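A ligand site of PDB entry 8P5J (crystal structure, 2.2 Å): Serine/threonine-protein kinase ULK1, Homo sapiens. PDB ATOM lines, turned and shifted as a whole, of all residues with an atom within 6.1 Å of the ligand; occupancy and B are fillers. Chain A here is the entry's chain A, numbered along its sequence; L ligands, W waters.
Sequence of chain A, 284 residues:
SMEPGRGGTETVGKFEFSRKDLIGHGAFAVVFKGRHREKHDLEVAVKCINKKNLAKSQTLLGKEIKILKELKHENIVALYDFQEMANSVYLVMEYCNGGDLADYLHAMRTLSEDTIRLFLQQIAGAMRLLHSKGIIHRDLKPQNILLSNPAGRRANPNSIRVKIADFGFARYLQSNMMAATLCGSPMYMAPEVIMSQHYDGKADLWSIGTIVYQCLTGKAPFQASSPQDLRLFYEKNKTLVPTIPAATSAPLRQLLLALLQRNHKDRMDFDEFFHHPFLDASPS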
ATOM      1  N   ILE A  23      14.480 -31.585 -22.437  1.00  0.00           N
ATOM      2  CA  ILE A  23      14.483 -30.180 -22.087  1.00  0.00           C
ATOM      3  C   ILE A  23      14.767 -30.086 -20.584  1.00  0.00           C
ATOM      4  O   ILE A  23      15.698 -29.409 -20.173  1.00  0.00           O
ATOM      5  CB  ILE A  23      13.169 -29.500 -22.503  1.00  0.00           C
ATOM      6  CG1 ILE A  23      13.132 -29.370 -24.028  1.00  0.00           C
ATOM      7  CG2 ILE A  23      12.971 -28.158 -21.817  1.00  0.00           C
ATOM      8  CD1 ILE A  23      11.827 -28.853 -24.621  1.00  0.00           C
ATOM      9  N   GLY A  24      14.020 -30.846 -19.777  1.00  0.00           N
ATOM     10  CA  GLY A  24      14.236 -30.854 -18.349  1.00  0.00           C
ATOM     11  C   GLY A  24      13.401 -31.913 -17.650  1.00  0.00           C
ATOM     12  O   GLY A  24      12.433 -32.386 -18.216  1.00  0.00           O
ATOM     13  N   HIS A  25      13.788 -32.229 -16.410  1.00  0.00           N
ATOM     14  CA  HIS A  25      13.261 -33.303 -15.607  1.00  0.00           C
ATOM     15  C   HIS A  25      12.914 -32.722 -14.249  1.00  0.00           C
ATOM     16  O   HIS A  25      13.727 -32.824 -13.355  1.00  0.00           O
ATOM     17  CB  HIS A  25      14.356 -34.376 -15.446  1.00  0.00           C
ATOM     18  CG  HIS A  25      13.964 -35.697 -14.864  1.00  0.00           C
ATOM     19  ND1 HIS A  25      14.040 -36.871 -15.604  1.00  0.00           N
ATOM     20  CD2 HIS A  25      13.533 -36.081 -13.633  1.00  0.00           C
ATOM     21  CE1 HIS A  25      13.642 -37.897 -14.862  1.00  0.00           C
ATOM     22  NE2 HIS A  25      13.332 -37.446 -13.656  1.00  0.00           N
ATOM     23  N   GLY A  26      11.753 -32.069 -14.142  1.00  0.00           N
ATOM     24  CA  GLY A  26      11.214 -31.631 -12.861  1.00  0.00           C
ATOM     25  C   GLY A  26      10.649 -32.801 -12.053  1.00  0.00           C
ATOM     26  O   GLY A  26      10.533 -33.908 -12.575  1.00  0.00           O
ATOM     27  N   ALA A  29       7.017 -33.358 -13.798  1.00  0.00           N
ATOM     28  CA  ALA A  29       6.926 -33.466 -15.242  1.00  0.00           C
ATOM     29  C   ALA A  29       8.323 -33.703 -15.801  1.00  0.00           C
ATOM     30  O   ALA A  29       9.297 -33.202 -15.268  1.00  0.00           O
ATOM     31  CB  ALA A  29       6.327 -32.201 -15.812  1.00  0.00           C
ATOM     32  N   VAL A  31      10.061 -33.172 -19.658  1.00  0.00           N
ATOM     33  CA  VAL A  31       9.753 -32.428 -20.859  1.00  0.00           C
ATOM     34  C   VAL A  31      10.810 -32.696 -21.919  1.00  0.00           C
ATOM     35  O   VAL A  31      11.997 -32.644 -21.605  1.00  0.00           O
ATOM     36  CB  VAL A  31       9.689 -30.916 -20.559  1.00  0.00           C
ATOM     37  CG1 VAL A  31       9.050 -30.189 -21.732  1.00  0.00           C
ATOM     38  CG2 VAL A  31       8.957 -30.645 -19.260  1.00  0.00           C
ATOM     39  N   ALA A  45       7.262 -28.649 -27.341  1.00  0.00           N
ATOM     40  CA  ALA A  45       7.750 -29.296 -26.141  1.00  0.00           C
ATOM     41  C   ALA A  45       6.672 -30.280 -25.695  1.00  0.00           C
ATOM     42  O   ALA A  45       5.499 -29.946 -25.697  1.00  0.00           O
ATOM     43  CB  ALA A  45       8.016 -28.255 -25.064  1.00  0.00           C
ATOM     44  N   VAL A  46       7.080 -31.477 -25.272  1.00  0.00           N
ATOM     45  CA  VAL A  46       6.102 -32.464 -24.866  1.00  0.00           C
ATOM     46  C   VAL A  46       6.342 -32.782 -23.421  1.00  0.00           C
ATOM     47  O   VAL A  46       7.406 -33.290 -23.087  1.00  0.00           O
ATOM     48  CB  VAL A  46       6.141 -33.731 -25.712  1.00  0.00           C
ATOM     49  CG1 VAL A  46       5.109 -34.725 -25.206  1.00  0.00           C
ATOM     50  CG2 VAL A  46       5.901 -33.411 -27.174  1.00  0.00           C
ATOM     51  N   LYS A  47       5.302 -32.558 -22.616  1.00  0.00           N
ATOM     52  CA  LYS A  47       5.358 -32.727 -21.165  1.00  0.00           C
ATOM     53  C   LYS A  47       4.739 -34.074 -20.816  1.00  0.00           C
ATOM     54  O   LYS A  47       3.652 -34.390 -21.257  1.00  0.00           O
ATOM     55  CB  LYS A  47       4.602 -31.513 -20.629  1.00  0.00           C
ATOM     56  CG  LYS A  47       5.187 -30.730 -19.482  1.00  0.00           C
ATOM     57  CD  LYS A  47       4.545 -29.335 -19.342  1.00  0.00           C
ATOM     58  CE  LYS A  47       5.116 -28.579 -18.167  1.00  0.00           C
ATOM     59  NZ  LYS A  47       4.202 -27.515 -17.706  1.00  0.00           N
ATOM     60  N   VAL A  77       2.536 -19.759 -22.399  1.00  0.00           N
ATOM     61  CA  VAL A  77       2.898 -20.930 -23.206  1.00  0.00           C
ATOM     62  C   VAL A  77       1.648 -21.653 -23.709  1.00  0.00           C
ATOM     63  O   VAL A  77       0.809 -22.038 -22.922  1.00  0.00           O
ATOM     64  CB  VAL A  77       3.801 -21.895 -22.434  1.00  0.00           C
ATOM     65  CG1 VAL A  77       4.322 -23.008 -23.332  1.00  0.00           C
ATOM     66  CG2 VAL A  77       5.017 -21.177 -21.877  1.00  0.00           C
ATOM     67  N   MET A  93       3.045 -28.598 -26.261  1.00  0.00           N
ATOM     68  CA  MET A  93       3.117 -27.172 -25.965  1.00  0.00           C
ATOM     69  C   MET A  93       4.092 -26.481 -26.901  1.00  0.00           C
ATOM     70  O   MET A  93       5.017 -27.093 -27.427  1.00  0.00           O
ATOM     71  CB  MET A  93       3.608 -27.020 -24.532  1.00  0.00           C
ATOM     72  CG  MET A  93       2.744 -27.823 -23.611  1.00  0.00           C
ATOM     73  SD  MET A  93       2.809 -27.316 -21.927  1.00  0.00           S
ATOM     74  CE  MET A  93       1.795 -25.848 -22.081  1.00  0.00           C
ATOM     75  N   GLU A  94       3.864 -25.185 -27.052  1.00  0.00           N
ATOM     76  CA  GLU A  94       4.800 -24.251 -27.675  1.00  0.00           C
ATOM     77  C   GLU A  94       6.167 -24.438 -27.049  1.00  0.00           C
ATOM     78  O   GLU A  94       6.303 -24.530 -25.828  1.00  0.00           O
ATOM     79  CB  GLU A  94       4.165 -22.875 -27.467  1.00  0.00           C
ATOM     80  CG  GLU A  94       5.031 -21.686 -27.733  1.00  0.00           C
ATOM     81  CD  GLU A  94       4.330 -20.356 -27.433  1.00  0.00           C
ATOM     82  OE1 GLU A  94       3.383 -20.298 -26.583  1.00  0.00           O
ATOM     83  OE2 GLU A  94       4.686 -19.372 -28.067  1.00  0.00           O
ATOM     84  N   TYR A  95       7.185 -24.574 -27.916  1.00  0.00           N
ATOM     85  CA  TYR A  95       8.574 -24.643 -27.478  1.00  0.00           C
ATOM     86  C   TYR A  95       9.074 -23.214 -27.227  1.00  0.00           C
ATOM     87  O   TYR A  95       8.873 -22.347 -28.051  1.00  0.00           O
ATOM     88  CB  TYR A  95       9.432 -25.300 -28.568  1.00  0.00           C
ATOM     89  CG  TYR A  95      10.913 -25.339 -28.296  1.00  0.00           C
ATOM     90  CD1 TYR A  95      11.407 -25.865 -27.132  1.00  0.00           C
ATOM     91  CD2 TYR A  95      11.828 -24.824 -29.210  1.00  0.00           C
ATOM     92  CE1 TYR A  95      12.760 -25.931 -26.878  1.00  0.00           C
ATOM     93  CE2 TYR A  95      13.196 -24.884 -28.979  1.00  0.00           C
ATOM     94  CZ  TYR A  95      13.660 -25.452 -27.818  1.00  0.00           C
ATOM     95  OH  TYR A  95      15.000 -25.473 -27.536  1.00  0.00           O
ATOM     96  N   CYS A  96       9.670 -22.990 -26.061  1.00  0.00           N
ATOM     97  CA  CYS A  96      10.256 -21.690 -25.727  1.00  0.00           C
ATOM     98  C   CYS A  96      11.785 -21.823 -25.796  1.00  0.00           C
ATOM     99  O   CYS A  96      12.402 -22.361 -24.889  1.00  0.00           O
ATOM    100  CB  CYS A  96       9.749 -21.237 -24.371  1.00  0.00           C
ATOM    101  SG  CYS A  96       7.945 -21.020 -24.362  1.00  0.00           S
ATOM    102  N   ASN A  97      12.359 -21.328 -26.885  1.00  0.00           N
ATOM    103  CA  ASN A  97      13.737 -21.601 -27.260  1.00  0.00           C
ATOM    104  C   ASN A  97      14.737 -20.814 -26.413  1.00  0.00           C
ATOM    105  O   ASN A  97      15.911 -21.160 -26.372  1.00  0.00           O
ATOM    106  CB  ASN A  97      13.938 -21.313 -28.760  1.00  0.00           C
ATOM    107  CG  ASN A  97      13.617 -19.898 -29.146  1.00  0.00           C
ATOM    108  OD1 ASN A  97      13.331 -19.031 -28.329  1.00  0.00           O
ATOM    109  ND2 ASN A  97      13.641 -19.633 -30.430  1.00  0.00           N
ATOM    110  N   GLY A  98      14.258 -19.816 -25.661  1.00  0.00           N
ATOM    111  CA  GLY A  98      15.145 -19.010 -24.812  1.00  0.00           C
ATOM    112  C   GLY A  98      15.378 -19.572 -23.411  1.00  0.00           C
ATOM    113  O   GLY A  98      16.161 -18.984 -22.646  1.00  0.00           O
ATOM    114  N   GLY A  99      14.672 -20.636 -23.033  1.00  0.00           N
ATOM    115  CA  GLY A  99      14.827 -21.153 -21.671  1.00  0.00           C
ATOM    116  C   GLY A  99      14.120 -20.260 -20.644  1.00  0.00           C
ATOM    117  O   GLY A  99      13.142 -19.616 -20.994  1.00  0.00           O
ATOM    118  N   ASP A 100      14.578 -20.288 -19.376  1.00  0.00           N
ATOM    119  CA  ASP A 100      13.855 -19.621 -18.309  1.00  0.00           C
ATOM    120  C   ASP A 100      14.542 -18.341 -17.832  1.00  0.00           C
ATOM    121  O   ASP A 100      15.740 -18.095 -18.053  1.00  0.00           O
ATOM    122  CB  ASP A 100      13.568 -20.550 -17.134  1.00  0.00           C
ATOM    123  CG  ASP A 100      14.775 -21.039 -16.382  1.00  0.00           C
ATOM    124  OD1 ASP A 100      15.902 -20.689 -16.776  1.00  0.00           O
ATOM    125  OD2 ASP A 100      14.581 -21.811 -15.402  1.00  0.00           O
ATOM    126  N   ASP A 103      17.691 -18.796 -15.455  1.00  0.00           N
ATOM    127  CA  ASP A 103      19.012 -18.958 -16.061  1.00  0.00           C
ATOM    128  C   ASP A 103      19.554 -17.604 -16.567  1.00  0.00           C
ATOM    129  O   ASP A 103      20.743 -17.285 -16.445  1.00  0.00           O
ATOM    130  CB  ASP A 103      18.965 -19.942 -17.225  1.00  0.00           C
ATOM    131  CG  ASP A 103      18.936 -21.434 -16.915  1.00  0.00           C
ATOM    132  OD1 ASP A 103      19.117 -21.816 -15.751  1.00  0.00           O
ATOM    133  OD2 ASP A 103      18.814 -22.204 -17.905  1.00  0.00           O
ATOM    134  N   GLN A 143      11.746 -19.654 -12.600  1.00  0.00           N
ATOM    135  CA  GLN A 143      11.802 -20.968 -13.225  1.00  0.00           C
ATOM    136  C   GLN A 143      10.557 -21.233 -14.077  1.00  0.00           C
ATOM    137  O   GLN A 143      10.616 -22.102 -14.934  1.00  0.00           O
ATOM    138  CB  GLN A 143      11.954 -22.090 -12.212  1.00  0.00           C
ATOM    139  CG  GLN A 143      13.253 -22.019 -11.415  1.00  0.00           C
ATOM    140  CD  GLN A 143      13.316 -20.965 -10.327  1.00  0.00           C
ATOM    141  OE1 GLN A 143      12.372 -20.242 -10.016  1.00  0.00           O
ATOM    142  NE2 GLN A 143      14.504 -20.807  -9.766  1.00  0.00           N
ATOM    143  N   ASN A 144       9.473 -20.479 -13.871  1.00  0.00           N
ATOM    144  CA  ASN A 144       8.225 -20.693 -14.585  1.00  0.00           C
ATOM    145  C   ASN A 144       7.922 -19.553 -15.519  1.00  0.00           C
ATOM    146  O   ASN A 144       6.789 -19.418 -15.993  1.00  0.00           O
ATOM    147  CB  ASN A 144       7.058 -20.870 -13.605  1.00  0.00           C
ATOM    148  CG  ASN A 144       7.136 -22.247 -12.971  1.00  0.00           C
ATOM    149  OD1 ASN A 144       7.711 -23.176 -13.553  1.00  0.00           O
ATOM    150  ND2 ASN A 144       6.494 -22.385 -11.823  1.00  0.00           N
ATOM    151  N   LEU A 146       9.293 -18.260 -19.069  1.00  0.00           N
ATOM    152  CA  LEU A 146      10.128 -18.757 -20.144  1.00  0.00           C
ATOM    153  C   LEU A 146      10.314 -17.626 -21.156  1.00  0.00           C
ATOM    154  O   LEU A 146       9.498 -16.706 -21.229  1.00  0.00           O
ATOM    155  CB  LEU A 146       9.504 -19.985 -20.783  1.00  0.00           C
ATOM    156  CG  LEU A 146       9.245 -21.179 -19.865  1.00  0.00           C
ATOM    157  CD1 LEU A 146       8.873 -22.416 -20.663  1.00  0.00           C
ATOM    158  CD2 LEU A 146      10.439 -21.467 -18.972  1.00  0.00           C
ATOM    159  N   ALA A 165       4.569 -20.181 -17.760  1.00  0.00           N
ATOM    160  CA  ALA A 165       4.417 -21.609 -17.844  1.00  0.00           C
ATOM    161  C   ALA A 165       4.005 -22.175 -16.491  1.00  0.00           C
ATOM    162  O   ALA A 165       3.971 -21.454 -15.491  1.00  0.00           O
ATOM    163  CB  ALA A 165       5.709 -22.205 -18.307  1.00  0.00           C
ATOM    164  N   ASP A 166       3.685 -23.473 -16.496  1.00  0.00           N
ATOM    165  CA  ASP A 166       3.513 -24.299 -15.301  1.00  0.00           C
ATOM    166  C   ASP A 166       2.251 -23.944 -14.536  1.00  0.00           C
ATOM    167  O   ASP A 166       2.318 -23.453 -13.416  1.00  0.00           O
ATOM    168  CB  ASP A 166       4.740 -24.225 -14.395  1.00  0.00           C
ATOM    169  CG  ASP A 166       5.568 -25.490 -14.481  1.00  0.00           C
ATOM    170  OD1 ASP A 166       6.132 -25.761 -15.562  1.00  0.00           O
ATOM    171  OD2 ASP A 166       5.586 -26.213 -13.467  1.00  0.00           O
HETATM  172  C1  LIG L   1      14.252 -28.222 -14.977  1.00  0.00           C
HETATM  173  C2  LIG L   1      13.947 -27.272 -16.119  1.00  0.00           C
HETATM  174  C3  LIG L   1      12.582 -27.443 -16.794  1.00  0.00           C
HETATM  175  C4  LIG L   1      10.574 -26.123 -17.349  1.00  0.00           C
HETATM  176  C5  LIG L   1      10.180 -26.715 -18.535  1.00  0.00           C
HETATM  177  C6  LIG L   1       8.993 -26.307 -19.081  1.00  0.00           C
HETATM  178  O1  LIG L   1      12.205 -28.461 -17.398  1.00  0.00           O
HETATM  179  O2  LIG L   1       8.572 -26.763 -20.312  1.00  0.00           O
HETATM  180  O3  LIG L   1      14.279 -24.611 -23.614  1.00  0.00           O
HETATM  181  N1  LIG L   1      11.766 -26.383 -16.663  1.00  0.00           N
HETATM  182  C7  LIG L   1       8.151 -25.432 -18.466  1.00  0.00           C
HETATM  183  C8  LIG L   1       8.534 -24.881 -17.253  1.00  0.00           C
HETATM  184  C9  LIG L   1       9.738 -25.245 -16.670  1.00  0.00           C
HETATM  185  C10 LIG L   1       8.977 -26.050 -21.397  1.00  0.00           C
HETATM  186  N2  LIG L   1      10.207 -25.593 -21.479  1.00  0.00           N
HETATM  187  C11 LIG L   1      10.546 -24.922 -22.581  1.00  0.00           C
HETATM  188  N3  LIG L   1       9.701 -24.656 -23.592  1.00  0.00           N
HETATM  189  C12 LIG L   1       8.461 -25.104 -23.480  1.00  0.00           C
HETATM  190  C13 LIG L   1       8.027 -25.817 -22.371  1.00  0.00           C
HETATM  191 CL1  LIG L   1       6.386 -26.414 -22.221  1.00  0.00          CL
HETATM  192  N4  LIG L   1      11.812 -24.461 -22.699  1.00  0.00           N
HETATM  193  C14 LIG L   1      12.865 -24.543 -21.769  1.00  0.00           C
HETATM  194  C15 LIG L   1      14.176 -24.645 -22.265  1.00  0.00           C
HETATM  195  C16 LIG L   1      15.225 -24.753 -21.378  1.00  0.00           C
HETATM  196  C17 LIG L   1      14.977 -24.712 -19.992  1.00  0.00           C
HETATM  197  C18 LIG L   1      13.660 -24.645 -19.533  1.00  0.00           C
HETATM  198  C19 LIG L   1      12.620 -24.557 -20.411  1.00  0.00           C
HETATM  199  N5  LIG L   1      16.018 -24.835 -19.053  1.00  0.00           N
HETATM  200  C20 LIG L   1      17.310 -25.370 -19.476  1.00  0.00           C
HETATM  201  C21 LIG L   1      18.405 -25.248 -18.455  1.00  0.00           C
HETATM  202  N6  LIG L   1      17.959 -25.316 -17.074  1.00  0.00           N
HETATM  203  C22 LIG L   1      16.961 -24.312 -16.781  1.00  0.00           C
HETATM  204  C23 LIG L   1      15.761 -24.394 -17.689  1.00  0.00           C
HETATM  205  C24 LIG L   1      19.113 -25.195 -16.143  1.00  0.00           C
HETATM  206  C25 LIG L   1      15.531 -24.268 -24.178  1.00  0.00           C
HETATM  207  O   HOH W   1      12.775 -23.709 -15.620  1.00  0.00           O
HETATM  208  O   HOH W   2      16.632 -22.612 -14.135  1.00  0.00           O
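Ile 23 touches the ligand.
CA of Gly 24 touches O1 of the ligand, 3.3 Å away.
Val 31 touches the ligand.
Ala 45 touches the ligand (CB to C12, 3.6 Å).
Met 93 touches the ligand (CB to CL1, 3.7 Å).
Glu 94 touches the ligand.
OH of Tyr 95 touches C25 of the ligand (3.6 Å).
O of Asn 97 touches C25 of the ligand, at 3.8 Å.
Gly 99 touches the ligand (CA to C15, 3.6 Å).
Asp 100 touches the ligand.
O of Gln 143 touches C9 of the ligand, at 3.7 Å.
CD1 of Leu 146 touches N2 of the ligand (3.5 Å).
Asp 166 touches the ligand (OD1 to C8, 3.1 Å).
Hydrophobic or aromatic side chains within 4 Å of the ligand: Ile 23, Val 31, Ala 45, Met 93, Tyr 95 and Leu 146.
Along chain A the residues within 4 Å of the ligand span positions 23 to 166.
Water W1 lies within hydrogen-bond range of the side-chain carboxylate (OD2) of Asp 100 (2.6 Å), the backbone carbonyl oxygen (O) of Gln 143 (2.8 Å) and a nitrogen (N1) of the ligand (3.0 Å).
Water W2 bridges OD2 of Asp 100 (2.5 Å) and OD1 of Asp 103 (3.1 Å).
OD2 of Asp 103 lies within salt-bridge range of N6 of the ligand (3.3 Å).
O of Cys 96 lies within hydrogen-bond range of N4 of the ligand (3.1 Å).
The backbone NH of Cys 96 lies within hydrogen-bond range of a nitrogen (N3) of the ligand (3.0 Å).
N of Ile 23 lies within hydrogen-bond range of O of Val 31, 2.8 Å away.
The backbone NH of Ala 45 is in hydrogen-bond range of the backbone carbonyl oxygen of Met 93, at 2.7 Å.
OD1 of Asp 166 is in salt-bridge range of NZ of Lys 47, 3.4 Å away.
N of Asp 103 lies within hydrogen-bond range of OD1 of Asp 100, at 2.9 Å.
The backbone NH of Val 31 sits at hydrogen-bond distance from the backbone carbonyl oxygen of Gly 24.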
